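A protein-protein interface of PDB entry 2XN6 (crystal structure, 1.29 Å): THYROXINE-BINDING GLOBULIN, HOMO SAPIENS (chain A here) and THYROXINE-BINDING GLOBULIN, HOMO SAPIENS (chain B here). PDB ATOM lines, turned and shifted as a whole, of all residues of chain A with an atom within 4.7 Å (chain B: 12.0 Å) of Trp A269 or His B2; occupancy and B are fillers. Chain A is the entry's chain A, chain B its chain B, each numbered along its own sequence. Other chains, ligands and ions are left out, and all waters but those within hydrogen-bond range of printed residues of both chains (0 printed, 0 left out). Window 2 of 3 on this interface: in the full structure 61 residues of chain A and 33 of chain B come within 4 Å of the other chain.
The backbone NH (N) of Asp A271 is in hydrogen-bond range of the backbone carbonyl oxygen (O) of Pro B3, 2.9 Å away. The backbone NH of Ile B5 sits at hydrogen-bond distance from the backbone carbonyl oxygen of Asp A271 (3.0 Å).
O of Asp A211 sits at hydrogen-bond distance from N of Val A270 (2.9 Å).
Among the printed residues, pairs that only touch across the chains: Met A210 with His B2, Trp A269 with His B2, Trp A269 with Pro B3, Val A270 with Pro B3, Val A270 with Ile B5 and Asp A271 with Ile B4.
Trp A269 touches two residues of chain B. No residue of chain B comes within 4 Å of Gln A212. Asp A271 touches just these residues of chain B: Pro B3 (2.9 Å), Ile B4 (3.4 Å) and Ile B5 (3.0 Å). Of the printed residues of chain A, Ile B4 touches Asp A271 (3.4 Å). Of the printed residues of chain A, Pro B3 touches Trp A269, Val A270 and Asp A271. Printed residues of chain A within 4 Å of Ile B5: Val A270 (3.7 Å) and Asp A271 (3.0 Å). His A215 touches none of the printed residues of chain B. Gln B6 touches none of the printed residues of chain A. The nearest residue of chain B that does not touch Trp A269 is Ile B4 (6.4 Å). The nearest residue of chain A that does not touch His B2 is Val A270 (4.6 Å).
Of the 5 printed residues of chain B, 4 touch a printed residue of chain A. Of the 8 printed residues of chain A, 4 touch a printed residue of chain B. Along chain A the printed residues that touch a printed residue of chain B span positions 210 to 271. Among the printed residues, 8 pairs touch across the chains.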
ATOM      1  N   MET A 210       1.611 -12.461  17.069  1.00  0.00           N
ATOM      2  CA  MET A 210       0.522 -13.376  17.345  1.00  0.00           C
ATOM      3  C   MET A 210       1.153 -14.743  17.566  1.00  0.00           C
ATOM      4  O   MET A 210       1.786 -15.294  16.666  1.00  0.00           O
ATOM      5  CB  MET A 210      -0.471 -13.392  16.186  1.00  0.00           C
ATOM      6  CG  MET A 210      -1.888 -13.798  16.596  1.00  0.00           C
ATOM      7  SD  MET A 210      -2.041 -15.527  17.103  1.00  0.00           S
ATOM      8  CE  MET A 210      -1.900 -16.352  15.520  1.00  0.00           C
ATOM      9  N   ASP A 211       1.003 -15.273  18.771  1.00  0.00           N
ATOM     10  CA  ASP A 211       1.640 -16.514  19.184  1.00  0.00           C
ATOM     11  C   ASP A 211       0.780 -17.201  20.251  1.00  0.00           C
ATOM     12  O   ASP A 211      -0.103 -16.563  20.845  1.00  0.00           O
ATOM     13  CB  ASP A 211       3.029 -16.186  19.749  1.00  0.00           C
ATOM     14  CG  ASP A 211       4.047 -17.272  19.475  1.00  0.00           C
ATOM     15  OD1 ASP A 211       3.958 -18.335  20.123  1.00  0.00           O
ATOM     16  OD2 ASP A 211       4.940 -17.058  18.619  1.00  0.00           O
ATOM     17  N   GLN A 212       1.057 -18.469  20.526  1.00  0.00           N
ATOM     18  CA  GLN A 212       0.432 -19.166  21.638  1.00  0.00           C
ATOM     19  C   GLN A 212       1.182 -18.774  22.896  1.00  0.00           C
ATOM     20  O   GLN A 212       2.403 -18.938  22.982  1.00  0.00           O
ATOM     21  CB  GLN A 212       0.470 -20.675  21.450  1.00  0.00           C
ATOM     22  CG  GLN A 212      -0.423 -21.166  20.319  1.00  0.00           C
ATOM     23  CD  GLN A 212      -0.473 -22.685  20.211  1.00  0.00           C
ATOM     24  OE1 GLN A 212       0.100 -23.405  21.036  1.00  0.00           O
ATOM     25  NE2 GLN A 212      -1.143 -23.178  19.184  1.00  0.00           N
ATOM     26  N   HIS A 215      -1.919 -17.710  29.280  1.00  0.00           N
ATOM     27  CA  HIS A 215      -2.567 -16.503  29.756  1.00  0.00           C
ATOM     28  C   HIS A 215      -3.854 -16.862  30.489  1.00  0.00           C
ATOM     29  O   HIS A 215      -4.331 -17.999  30.416  1.00  0.00           O
ATOM     30  CB  HIS A 215      -2.841 -15.535  28.592  1.00  0.00           C
ATOM     31  CG  HIS A 215      -3.890 -16.012  27.641  1.00  0.00           C
ATOM     32  ND1 HIS A 215      -3.668 -16.995  26.703  1.00  0.00           N
ATOM     33  CD2 HIS A 215      -5.180 -15.633  27.493  1.00  0.00           C
ATOM     34  CE1 HIS A 215      -4.780 -17.200  26.019  1.00  0.00           C
ATOM     35  NE2 HIS A 215      -5.710 -16.383  26.476  1.00  0.00           N
ATOM     36  N   GLY A 268      -2.795 -20.534  24.632  1.00  0.00           N
ATOM     37  CA  GLY A 268      -3.661 -20.346  23.480  1.00  0.00           C
ATOM     38  C   GLY A 268      -3.218 -19.150  22.662  1.00  0.00           C
ATOM     39  O   GLY A 268      -2.404 -18.341  23.124  1.00  0.00           O
ATOM     40  N   TRP A 269      -3.761 -19.016  21.457  1.00  0.00           N
ATOM     41  CA  TRP A 269      -3.405 -17.907  20.573  1.00  0.00           C
ATOM     42  C   TRP A 269      -3.760 -16.562  21.188  1.00  0.00           C
ATOM     43  O   TRP A 269      -4.859 -16.376  21.708  1.00  0.00           O
ATOM     44  CB  TRP A 269      -4.124 -18.023  19.232  1.00  0.00           C
ATOM     45  CG  TRP A 269      -3.825 -19.270  18.498  1.00  0.00           C
ATOM     46  CD1 TRP A 269      -4.642 -20.347  18.349  1.00  0.00           C
ATOM     47  CD2 TRP A 269      -2.607 -19.590  17.829  1.00  0.00           C
ATOM     48  NE1 TRP A 269      -4.016 -21.316  17.611  1.00  0.00           N
ATOM     49  CE2 TRP A 269      -2.761 -20.882  17.284  1.00  0.00           C
ATOM     50  CE3 TRP A 269      -1.405 -18.911  17.627  1.00  0.00           C
ATOM     51  CZ2 TRP A 269      -1.755 -21.509  16.547  1.00  0.00           C
ATOM     52  CZ3 TRP A 269      -0.397 -19.540  16.893  1.00  0.00           C
ATOM     53  CH2 TRP A 269      -0.587 -20.826  16.370  1.00  0.00           C
ATOM     54  N   VAL A 270      -2.833 -15.619  21.079  1.00  0.00           N
ATOM     55  CA  VAL A 270      -3.022 -14.252  21.556  1.00  0.00           C
ATOM     56  C   VAL A 270      -2.389 -13.322  20.530  1.00  0.00           C
ATOM     57  O   VAL A 270      -1.255 -13.560  20.089  1.00  0.00           O
ATOM     58  CB  VAL A 270      -2.341 -14.008  22.931  1.00  0.00           C
ATOM     59  CG1 VAL A 270      -2.453 -12.534  23.347  1.00  0.00           C
ATOM     60  CG2 VAL A 270      -2.924 -14.907  24.007  1.00  0.00           C
ATOM     61  N   ASP A 271      -3.125 -12.282  20.147  1.00  0.00           N
ATOM     62  CA  ASP A 271      -2.581 -11.171  19.375  1.00  0.00           C
ATOM     63  C   ASP A 271      -2.018 -10.192  20.400  1.00  0.00           C
ATOM     64  O   ASP A 271      -2.760  -9.470  21.049  1.00  0.00           O
ATOM     65  CB  ASP A 271      -3.698 -10.533  18.545  1.00  0.00           C
ATOM     66  CG  ASP A 271      -3.187  -9.606  17.465  1.00  0.00           C
ATOM     67  OD1 ASP A 271      -1.969  -9.579  17.203  1.00  0.00           O
ATOM     68  OD2 ASP A 271      -4.029  -8.906  16.862  1.00  0.00           O
ATOM     69  N   HIS B   2      -8.683 -14.351  17.380  1.00  0.00           N
ATOM     70  CA  HIS B   2      -7.947 -14.655  18.640  1.00  0.00           C
ATOM     71  C   HIS B   2      -8.016 -13.458  19.575  1.00  0.00           C
ATOM     72  O   HIS B   2      -8.095 -12.320  19.107  1.00  0.00           O
ATOM     73  CB  HIS B   2      -6.479 -14.975  18.346  1.00  0.00           C
ATOM     74  CG  HIS B   2      -6.283 -16.010  17.285  1.00  0.00           C
ATOM     75  ND1 HIS B   2      -6.792 -17.286  17.390  1.00  0.00           N
ATOM     76  CD2 HIS B   2      -5.618 -15.966  16.107  1.00  0.00           C
ATOM     77  CE1 HIS B   2      -6.459 -17.980  16.317  1.00  0.00           C
ATOM     78  NE2 HIS B   2      -5.745 -17.203  15.523  1.00  0.00           N
ATOM     79  N   PRO B   3      -7.974 -13.701  20.898  1.00  0.00           N
ATOM     80  CA  PRO B   3      -8.008 -12.595  21.848  1.00  0.00           C
ATOM     81  C   PRO B   3      -6.826 -11.649  21.677  1.00  0.00           C
ATOM     82  O   PRO B   3      -5.713 -12.089  21.371  1.00  0.00           O
ATOM     83  CB  PRO B   3      -7.930 -13.294  23.212  1.00  0.00           C
ATOM     84  CG  PRO B   3      -7.354 -14.621  22.927  1.00  0.00           C
ATOM     85  CD  PRO B   3      -7.860 -14.998  21.585  1.00  0.00           C
ATOM     86  N   ILE B   4      -7.080 -10.361  21.877  1.00  0.00           N
ATOM     87  CA  ILE B   4      -6.046  -9.339  21.841  1.00  0.00           C
ATOM     88  C   ILE B   4      -5.653  -8.985  23.266  1.00  0.00           C
ATOM     89  O   ILE B   4      -6.516  -8.741  24.111  1.00  0.00           O
ATOM     90  CB  ILE B   4      -6.547  -8.071  21.124  1.00  0.00           C
ATOM     91  CG1 ILE B   4      -6.841  -8.375  19.655  1.00  0.00           C
ATOM     92  CG2 ILE B   4      -5.518  -6.964  21.214  1.00  0.00           C
ATOM     93  CD1 ILE B   4      -7.712  -7.339  18.978  1.00  0.00           C
ATOM     94  N   ILE B   5      -4.351  -8.980  23.534  1.00  0.00           N
ATOM     95  CA  ILE B   5      -3.832  -8.417  24.776  1.00  0.00           C
ATOM     96  C   ILE B   5      -2.910  -7.265  24.386  1.00  0.00           C
ATOM     97  O   ILE B   5      -1.897  -7.466  23.697  1.00  0.00           O
ATOM     98  CB  ILE B   5      -3.095  -9.466  25.636  1.00  0.00           C
ATOM     99  CG1 ILE B   5      -4.069 -10.570  26.064  1.00  0.00           C
ATOM    100  CG2 ILE B   5      -2.467  -8.803  26.862  1.00  0.00           C
ATOM    101  CD1 ILE B   5      -3.442 -11.672  26.886  1.00  0.00           C
ATOM    102  N   GLN B   6      -3.295  -6.056  24.789  1.00  0.00           N
ATOM    103  CA  GLN B   6      -2.538  -4.847  24.482  1.00  0.00           C
ATOM    104  C   GLN B   6      -1.994  -4.261  25.767  1.00  0.00           C
ATOM    105  O   GLN B   6      -2.753  -3.706  26.557  1.00  0.00           O
ATOM    106  CB  GLN B   6      -3.440  -3.807  23.826  1.00  0.00           C
ATOM    107  CG  GLN B   6      -3.728  -4.033  22.378  1.00  0.00           C
ATOM    108  CD  GLN B   6      -4.465  -2.858  21.776  1.00  0.00           C
ATOM    109  OE1 GLN B   6      -3.878  -2.040  21.064  1.00  0.00           O
ATOM    110  NE2 GLN B   6      -5.744  -2.741  22.095  1.00  0.00           N
